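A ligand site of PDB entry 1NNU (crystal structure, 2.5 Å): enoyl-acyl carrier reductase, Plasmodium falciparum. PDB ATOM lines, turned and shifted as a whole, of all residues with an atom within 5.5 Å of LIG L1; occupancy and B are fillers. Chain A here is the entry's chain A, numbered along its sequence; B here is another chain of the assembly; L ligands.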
ATOM      1  N   LEU A 120      26.965   6.745   5.179  1.00  0.00           N
ATOM      2  CA  LEU A 120      26.541   7.146   6.509  1.00  0.00           C
ATOM      3  C   LEU A 120      25.024   7.234   6.595  1.00  0.00           C
ATOM      4  O   LEU A 120      24.336   7.446   5.588  1.00  0.00           O
ATOM      5  CB  LEU A 120      27.153   8.509   6.852  1.00  0.00           C
ATOM      6  CG  LEU A 120      26.671   9.714   6.032  1.00  0.00           C
ATOM      7  CD1 LEU A 120      25.834  10.631   6.915  1.00  0.00           C
ATOM      8  CD2 LEU A 120      27.847  10.478   5.489  1.00  0.00           C
ATOM      9  N   ALA A 121      24.498   7.077   7.794  1.00  0.00           N
ATOM     10  CA  ALA A 121      23.067   7.163   8.037  1.00  0.00           C
ATOM     11  C   ALA A 121      22.882   7.577   9.487  1.00  0.00           C
ATOM     12  O   ALA A 121      23.776   7.405  10.309  1.00  0.00           O
ATOM     13  CB  ALA A 121      22.401   5.814   7.766  1.00  0.00           C
ATOM     14  N   ASN A 122      21.722   8.143   9.798  1.00  0.00           N
ATOM     15  CA  ASN A 122      21.455   8.552  11.164  1.00  0.00           C
ATOM     16  C   ASN A 122      19.982   8.822  11.358  1.00  0.00           C
ATOM     17  O   ASN A 122      19.379   9.596  10.623  1.00  0.00           O
ATOM     18  CB  ASN A 122      22.275   9.804  11.514  1.00  0.00           C
ATOM     19  CG  ASN A 122      22.363  10.042  13.010  1.00  0.00           C
ATOM     20  OD1 ASN A 122      21.432  10.551  13.631  1.00  0.00           O
ATOM     21  ND2 ASN A 122      23.491   9.660  13.590  1.00  0.00           N
ATOM     22  N   ALA A 123      19.408   8.146  12.347  1.00  0.00           N
ATOM     23  CA  ALA A 123      17.990   8.306  12.655  1.00  0.00           C
ATOM     24  C   ALA A 123      17.792   8.214  14.165  1.00  0.00           C
ATOM     25  O   ALA A 123      17.805   7.130  14.739  1.00  0.00           O
ATOM     26  CB  ALA A 123      17.178   7.221  11.939  1.00  0.00           C
ATOM     27  N   LYS A 124      17.625   9.366  14.802  1.00  0.00           N
ATOM     28  CA  LYS A 124      17.427   9.421  16.254  1.00  0.00           C
ATOM     29  C   LYS A 124      16.337   8.495  16.779  1.00  0.00           C
ATOM     30  O   LYS A 124      16.431   8.001  17.897  1.00  0.00           O
ATOM     31  CB  LYS A 124      17.075  10.845  16.695  1.00  0.00           C
ATOM     32  CG  LYS A 124      18.240  11.819  16.727  1.00  0.00           C
ATOM     33  CD  LYS A 124      17.745  13.191  17.192  1.00  0.00           C
ATOM     34  CE  LYS A 124      18.869  14.223  17.210  1.00  0.00           C
ATOM     35  NZ  LYS A 124      18.360  15.575  17.603  1.00  0.00           N
ATOM     36  N   VAL A 126      15.119   5.532  15.227  1.00  0.00           N
ATOM     37  CA  VAL A 126      15.057   4.250  14.526  1.00  0.00           C
ATOM     38  C   VAL A 126      14.319   3.163  15.313  1.00  0.00           C
ATOM     39  O   VAL A 126      13.832   2.188  14.740  1.00  0.00           O
ATOM     40  CB  VAL A 126      16.471   3.735  14.179  1.00  0.00           C
ATOM     41  CG1 VAL A 126      17.191   3.280  15.436  1.00  0.00           C
ATOM     42  CG2 VAL A 126      16.381   2.616  13.168  1.00  0.00           C
ATOM     43  N   TYR A 171      19.092   0.402   1.605  1.00  0.00           N
ATOM     44  CA  TYR A 171      18.570  -0.860   2.092  1.00  0.00           C
ATOM     45  C   TYR A 171      17.198  -1.072   1.484  1.00  0.00           C
ATOM     46  O   TYR A 171      16.419  -0.131   1.352  1.00  0.00           O
ATOM     47  CB  TYR A 171      18.499  -0.827   3.628  1.00  0.00           C
ATOM     48  CG  TYR A 171      18.043  -2.115   4.272  1.00  0.00           C
ATOM     49  CD1 TYR A 171      18.638  -3.325   3.926  1.00  0.00           C
ATOM     50  CD2 TYR A 171      17.016  -2.130   5.207  1.00  0.00           C
ATOM     51  CE1 TYR A 171      18.210  -4.522   4.493  1.00  0.00           C
ATOM     52  CE2 TYR A 171      16.578  -3.322   5.781  1.00  0.00           C
ATOM     53  CZ  TYR A 171      17.183  -4.516   5.415  1.00  0.00           C
ATOM     54  OH  TYR A 171      16.733  -5.706   5.946  1.00  0.00           O
ATOM     55  N   TYR A 181      12.889  -1.397  11.154  1.00  0.00           N
ATOM     56  CA  TYR A 181      13.661  -0.359  10.481  1.00  0.00           C
ATOM     57  C   TYR A 181      12.816   0.907  10.513  1.00  0.00           C
ATOM     58  O   TYR A 181      12.350   1.385   9.479  1.00  0.00           O
ATOM     59  CB  TYR A 181      13.888  -0.778   9.028  1.00  0.00           C
ATOM     60  CG  TYR A 181      15.031  -0.076   8.324  1.00  0.00           C
ATOM     61  CD1 TYR A 181      16.359  -0.289   8.712  1.00  0.00           C
ATOM     62  CD2 TYR A 181      14.790   0.787   7.260  1.00  0.00           C
ATOM     63  CE1 TYR A 181      17.411   0.333   8.044  1.00  0.00           C
ATOM     64  CE2 TYR A 181      15.834   1.411   6.580  1.00  0.00           C
ATOM     65  CZ  TYR A 181      17.141   1.175   6.977  1.00  0.00           C
ATOM     66  OH  TYR A 181      18.182   1.756   6.291  1.00  0.00           O
ATOM     67  N   MET A 185      14.006   5.742   8.637  1.00  0.00           N
ATOM     68  CA  MET A 185      15.147   5.273   7.862  1.00  0.00           C
ATOM     69  C   MET A 185      14.615   4.826   6.512  1.00  0.00           C
ATOM     70  O   MET A 185      15.146   5.205   5.471  1.00  0.00           O
ATOM     71  CB  MET A 185      15.838   4.088   8.549  1.00  0.00           C
ATOM     72  CG  MET A 185      16.971   4.506   9.471  1.00  0.00           C
ATOM     73  SD  MET A 185      18.139   5.620   8.649  1.00  0.00           S
ATOM     74  CE  MET A 185      18.716   4.564   7.363  1.00  0.00           C
ATOM     75  N   LYS A 189      15.819   6.159   2.953  1.00  0.00           N
ATOM     76  CA  LYS A 189      16.422   5.302   1.943  1.00  0.00           C
ATOM     77  C   LYS A 189      15.640   5.413   0.636  1.00  0.00           C
ATOM     78  O   LYS A 189      16.215   5.323  -0.452  1.00  0.00           O
ATOM     79  CB  LYS A 189      16.472   3.856   2.434  1.00  0.00           C
ATOM     80  CG  LYS A 189      17.450   3.628   3.583  1.00  0.00           C
ATOM     81  CD  LYS A 189      18.854   4.134   3.212  1.00  0.00           C
ATOM     82  CE  LYS A 189      19.886   3.763   4.264  1.00  0.00           C
ATOM     83  NZ  LYS A 189      21.243   4.289   3.944  1.00  0.00           N
ATOM     84  N   PRO A 218      22.390  -7.545   5.001  1.00  0.00           N
ATOM     85  CA  PRO A 218      22.700  -7.310   6.421  1.00  0.00           C
ATOM     86  C   PRO A 218      24.169  -7.482   6.777  1.00  0.00           C
ATOM     87  O   PRO A 218      24.838  -8.377   6.262  1.00  0.00           O
ATOM     88  CB  PRO A 218      21.830  -8.351   7.141  1.00  0.00           C
ATOM     89  CG  PRO A 218      20.897  -8.895   6.084  1.00  0.00           C
ATOM     90  CD  PRO A 218      21.700  -8.836   4.841  1.00  0.00           C
ATOM     91  N   LEU A 219      24.660  -6.619   7.650  1.00  0.00           N
ATOM     92  CA  LEU A 219      26.041  -6.677   8.110  1.00  0.00           C
ATOM     93  C   LEU A 219      26.048  -6.259   9.581  1.00  0.00           C
ATOM     94  O   LEU A 219      25.581  -5.172   9.932  1.00  0.00           O
ATOM     95  CB  LEU A 219      26.914  -5.707   7.298  1.00  0.00           C
ATOM     96  CG  LEU A 219      28.387  -5.598   7.711  1.00  0.00           C
ATOM     97  CD1 LEU A 219      29.165  -6.812   7.212  1.00  0.00           C
ATOM     98  CD2 LEU A 219      28.987  -4.329   7.124  1.00  0.00           C
ATOM     99  N   SER A 221      27.260  -4.464  11.807  1.00  0.00           N
ATOM    100  CA  SER A 221      28.124  -3.311  12.033  1.00  0.00           C
ATOM    101  C   SER A 221      27.739  -2.678  13.372  1.00  0.00           C
ATOM    102  O   SER A 221      26.755  -3.081  13.994  1.00  0.00           O
ATOM    103  CB  SER A 221      27.956  -2.287  10.899  1.00  0.00           C
ATOM    104  OG  SER A 221      26.640  -1.758  10.852  1.00  0.00           O
ATOM    105  N   ALA A 223      26.484   0.312  14.024  1.00  0.00           N
ATOM    106  CA  ALA A 223      25.198   0.976  13.914  1.00  0.00           C
ATOM    107  C   ALA A 223      24.055  -0.031  13.828  1.00  0.00           C
ATOM    108  O   ALA A 223      22.953   0.234  14.319  1.00  0.00           O
ATOM    109  CB  ALA A 223      25.179   1.885  12.697  1.00  0.00           C
ATOM    110  N   ALA A 224      24.315  -1.164  13.193  1.00  0.00           N
ATOM    111  CA  ALA A 224      23.303  -2.203  13.042  1.00  0.00           C
ATOM    112  C   ALA A 224      22.891  -2.726  14.406  1.00  0.00           C
ATOM    113  O   ALA A 224      21.712  -2.948  14.667  1.00  0.00           O
ATOM    114  CB  ALA A 224      23.844  -3.349  12.189  1.00  0.00           C
ATOM    115  N   ALA A 226      22.774  -1.152  17.042  1.00  0.00           N
ATOM    116  CA  ALA A 226      21.948  -0.128  17.648  1.00  0.00           C
ATOM    117  C   ALA A 226      20.461  -0.411  17.458  1.00  0.00           C
ATOM    118  O   ALA A 226      19.683  -0.358  18.415  1.00  0.00           O
ATOM    119  CB  ALA A 226      22.287   1.229  17.058  1.00  0.00           C
ATOM    120  N   ILE A 227      20.062  -0.697  16.223  1.00  0.00           N
ATOM    121  CA  ILE A 227      18.666  -0.979  15.915  1.00  0.00           C
ATOM    122  C   ILE A 227      18.125  -2.091  16.809  1.00  0.00           C
ATOM    123  O   ILE A 227      18.226  -3.274  16.481  1.00  0.00           O
ATOM    124  CB  ILE A 227      18.497  -1.420  14.450  1.00  0.00           C
ATOM    125  CG1 ILE A 227      19.161  -0.410  13.517  1.00  0.00           C
ATOM    126  CG2 ILE A 227      17.015  -1.563  14.121  1.00  0.00           C
ATOM    127  CD1 ILE A 227      19.076  -0.766  12.056  1.00  0.00           C
ATOM    128  N   PHE B   3      17.470  -7.026  16.111  1.00  0.00           N
ATOM    129  CA  PHE B   3      17.058  -6.931  14.725  1.00  0.00           C
ATOM    130  C   PHE B   3      18.073  -7.410  13.705  1.00  0.00           C
ATOM    131  O   PHE B   3      17.734  -8.151  12.781  1.00  0.00           O
ATOM    132  CB  PHE B   3      16.674  -5.486  14.423  1.00  0.00           C
ATOM    133  CG  PHE B   3      16.623  -5.158  12.966  1.00  0.00           C
ATOM    134  CD1 PHE B   3      15.619  -5.661  12.158  1.00  0.00           C
ATOM    135  CD2 PHE B   3      17.602  -4.353  12.396  1.00  0.00           C
ATOM    136  CE1 PHE B   3      15.585  -5.376  10.800  1.00  0.00           C
ATOM    137  CE2 PHE B   3      17.584  -4.053  11.039  1.00  0.00           C
ATOM    138  CZ  PHE B   3      16.572  -4.574  10.242  1.00  0.00           C
ATOM    139  N   ILE B   4      19.325  -6.987  13.860  1.00  0.00           N
ATOM    140  CA  ILE B   4      20.355  -7.360  12.901  1.00  0.00           C
ATOM    141  C   ILE B   4      20.648  -8.843  12.897  1.00  0.00           C
ATOM    142  O   ILE B   4      20.920  -9.417  11.838  1.00  0.00           O
ATOM    143  CB  ILE B   4      21.675  -6.582  13.146  1.00  0.00           C
ATOM    144  CG1 ILE B   4      22.616  -6.775  11.947  1.00  0.00           C
ATOM    145  CG2 ILE B   4      22.363  -7.089  14.414  1.00  0.00           C
ATOM    146  CD1 ILE B   4      22.058  -6.235  10.635  1.00  0.00           C
ATOM    147  N   ALA B   7      17.899 -10.549  10.805  1.00  0.00           N
ATOM    148  CA  ALA B   7      18.099 -10.315   9.380  1.00  0.00           C
ATOM    149  C   ALA B   7      19.239 -11.166   8.824  1.00  0.00           C
ATOM    150  O   ALA B   7      19.081 -11.812   7.775  1.00  0.00           O
ATOM    151  CB  ALA B   7      18.378  -8.839   9.132  1.00  0.00           C
HETATM  152  C1  LIG L   1      23.272   4.119  10.741  1.00  0.00           C
HETATM  153  C2  LIG L   1      23.379   3.060   9.827  1.00  0.00           C
HETATM  154  C3  LIG L   1      22.397   2.037   9.770  1.00  0.00           C
HETATM  155  C4  LIG L   1      21.260   2.070  10.640  1.00  0.00           C
HETATM  156  C5  LIG L   1      21.128   3.129  11.570  1.00  0.00           C
HETATM  157  C6  LIG L   1      22.170   4.194  11.622  1.00  0.00           C
HETATM  158  C7  LIG L   1      22.039   5.252  12.543  1.00  0.00           C
HETATM  159  C8  LIG L   1      20.934   5.306  13.405  1.00  0.00           C
HETATM  160  O1  LIG L   1      20.833   6.340  14.293  1.00  0.00           O
HETATM  161  C9  LIG L   1      19.933   4.301  13.364  1.00  0.00           C
HETATM  162  C10 LIG L   1      20.020   3.217  12.449  1.00  0.00           C
HETATM  163  O2  LIG L   1      22.618   1.007   8.830  1.00  0.00           O
HETATM  164  C11 LIG L   1      21.812  -0.124   8.621  1.00  0.00           C
HETATM  165  C12 LIG L   1      21.976  -1.260   9.481  1.00  0.00           C
HETATM  166  C13 LIG L   1      21.215  -2.439   9.286  1.00  0.00           C
HETATM  167  C14 LIG L   1      20.266  -2.517   8.241  1.00  0.00           C
HETATM  168 CL1  LIG L   1      19.339  -3.989   8.013  1.00  0.00          CL
HETATM  169  C15 LIG L   1      20.079  -1.383   7.387  1.00  0.00           C
HETATM  170  C16 LIG L   1      20.847  -0.185   7.581  1.00  0.00           C
HETATM  171  O3  LIG L   1      20.665   0.884   6.746  1.00  0.00           O
HETATM  172  P1  LG2 L   2      28.475   2.212  10.240  1.00  0.00           P
HETATM  173  O1  LG2 L   2      29.924   1.898  10.078  1.00  0.00           O
HETATM  174  O2  LG2 L   2      27.896   2.237  11.642  1.00  0.00           O
HETATM  175  O3  LG2 L   2      28.299   3.660   9.523  1.00  0.00           O
HETATM  176  C1  LG2 L   2      27.552   4.806   9.964  1.00  0.00           C
HETATM  177  C2  LG2 L   2      28.473   5.954  10.118  1.00  0.00           C
HETATM  178  O4  LG2 L   2      27.840   7.251   9.865  1.00  0.00           O
HETATM  179  C3  LG2 L   2      29.063   6.029  11.523  1.00  0.00           C
HETATM  180  O5  LG2 L   2      30.440   5.574  11.408  1.00  0.00           O
HETATM  181  C4  LG2 L   2      28.932   7.487  11.956  1.00  0.00           C
HETATM  182  O6  LG2 L   2      30.140   7.920  12.541  1.00  0.00           O
HETATM  183  C5  LG2 L   2      28.492   8.240  10.658  1.00  0.00           C
HETATM  184  N1  LG2 L   2      27.513   9.322  10.905  1.00  0.00           N
HETATM  185  C6  LG2 L   2      26.289   9.596  11.476  1.00  0.00           C
HETATM  186  N2  LG2 L   2      25.871  10.843  11.407  1.00  0.00           N
HETATM  187  C7  LG2 L   2      26.900  11.483  10.723  1.00  0.00           C
HETATM  188  C8  LG2 L   2      27.086  12.804  10.337  1.00  0.00           C
HETATM  189  N3  LG2 L   2      26.212  13.772  10.605  1.00  0.00           N
HETATM  190  N4  LG2 L   2      28.212  13.129   9.676  1.00  0.00           N
HETATM  191  C9  LG2 L   2      29.095  12.153   9.349  1.00  0.00           C
HETATM  192  N5  LG2 L   2      29.088  10.872   9.729  1.00  0.00           N
HETATM  193  C10 LG2 L   2      27.922  10.562  10.402  1.00  0.00           C
HETATM  194  O7  LG2 L   2      27.409   1.305   9.644  1.00  0.00           O
HETATM  195  P2  LG2 L   2      27.167   0.727   8.287  1.00  0.00           P
HETATM  196  O8  LG2 L   2      28.397   0.210   7.624  1.00  0.00           O
HETATM  197  O9  LG2 L   2      26.018  -0.185   8.495  1.00  0.00           O
HETATM  198  O10 LG2 L   2      26.403   1.914   7.536  1.00  0.00           O
HETATM  199  C11 LG2 L   2      26.931   2.622   6.413  1.00  0.00           C
HETATM  200  C12 LG2 L   2      25.859   2.684   5.320  1.00  0.00           C
HETATM  201  O11 LG2 L   2      25.503   1.335   4.865  1.00  0.00           O
HETATM  202  C13 LG2 L   2      24.585   3.360   5.844  1.00  0.00           C
HETATM  203  O12 LG2 L   2      24.197   4.295   4.879  1.00  0.00           O
HETATM  204  C14 LG2 L   2      23.644   2.212   5.942  1.00  0.00           C
HETATM  205  O13 LG2 L   2      22.328   2.652   5.844  1.00  0.00           O
HETATM  206  C15 LG2 L   2      24.071   1.349   4.780  1.00  0.00           C
HETATM  207  N6  LG2 L   2      23.534  -0.022   4.788  1.00  0.00           N
HETATM  208  C16 LG2 L   2      23.918  -0.886   5.846  1.00  0.00           C
HETATM  209  C17 LG2 L   2      23.500  -2.192   6.070  1.00  0.00           C
HETATM  210  C18 LG2 L   2      23.907  -3.096   7.156  1.00  0.00           C
HETATM  211  O14 LG2 L   2      23.306  -4.267   7.404  1.00  0.00           O
HETATM  212  N7  LG2 L   2      24.848  -2.832   8.044  1.00  0.00           N
HETATM  213  C19 LG2 L   2      22.704  -2.608   4.999  1.00  0.00           C
HETATM  214  C20 LG2 L   2      22.320  -1.857   3.843  1.00  0.00           C
HETATM  215  C21 LG2 L   2      22.755  -0.484   3.757  1.00  0.00           C
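O3 of LIG L1 is in hydrogen-bond range of OH of Tyr 181. The backbone NH (N) of Ala 123 lies within hydrogen-bond range of an oxygen (O1) of LIG L1 (3.0 Å). O1 of LIG L1 sits at hydrogen-bond distance from O of Ala 123, 3.2 Å away. The backbone NH of Ala 223 sits close to an oxygen (O2) of LG2 L2 (3.4 Å). ND2 of Asn 122 sits at hydrogen-bond distance from N2 of LG2 L2 (3.4 Å). An oxygen (O13) of LG2 L2 sits at hydrogen-bond distance from the side-chain amino group (NZ) of Lys 189, at 2.7 Å. An oxygen (O9) of LG2 L2 lies within hydrogen-bond range of the side-chain hydroxyl (OG) of Ser 221 (2.9 Å). N of Leu 219 lies within hydrogen-bond range of O14 of LG2 L2, at 2.7 Å. The backbone carbonyl oxygen of Leu 219 is in hydrogen-bond range of a nitrogen (N7) of LG2 L2, 3.1 Å away. An oxygen (O12) of LG2 L2 lies within hydrogen-bond range of the backbone carbonyl oxygen of Leu 120, at 3.2 Å.
O3 of LIG L1 is in hydrogen-bond range of O13 of LG2 L2 (2.6 Å).
The side-chain hydroxyl (OG) of Ser 221 is in hydrogen-bond range of the backbone NH (N) of Ala 224 (3.4 Å).
Ala 121 touches LIG L1 (O to C1, 3.4 Å). Asn 122 touches LIG L1 (CA to C7, 3.6 Å). Val 126 touches LIG L1 (CG1 to C9, 3.6 Å). CZ of Tyr 171 touches CL1 of LIG L1, at 3.4 Å. Lys 189 touches LIG L1 (CE to O3, 3.9 Å). Ala 223 touches LIG L1 (CB to C1, 3.5 Å). Ala 224 touches LIG L1 (CB to C12, 3.9 Å). Ile 227 touches LIG L1. Phe 3 of chain B touches LIG L1 (CE2 to CL1, 3.5 Å). Hydrophobic or aromatic side chains that line LIG L1: Ala 121, Val 126, Tyr 171, Tyr 181, Ala 223, Ala 224, Ile 227 and Phe 3 of chain B. 11 residues have an atom within 4 Å of LIG L1: Ala 121, Asn 122, Ala 123, Val 126, Tyr 171, Tyr 181, Lys 189, Ala 223, Ala 224, Ile 227 and Phe 3 of chain B.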
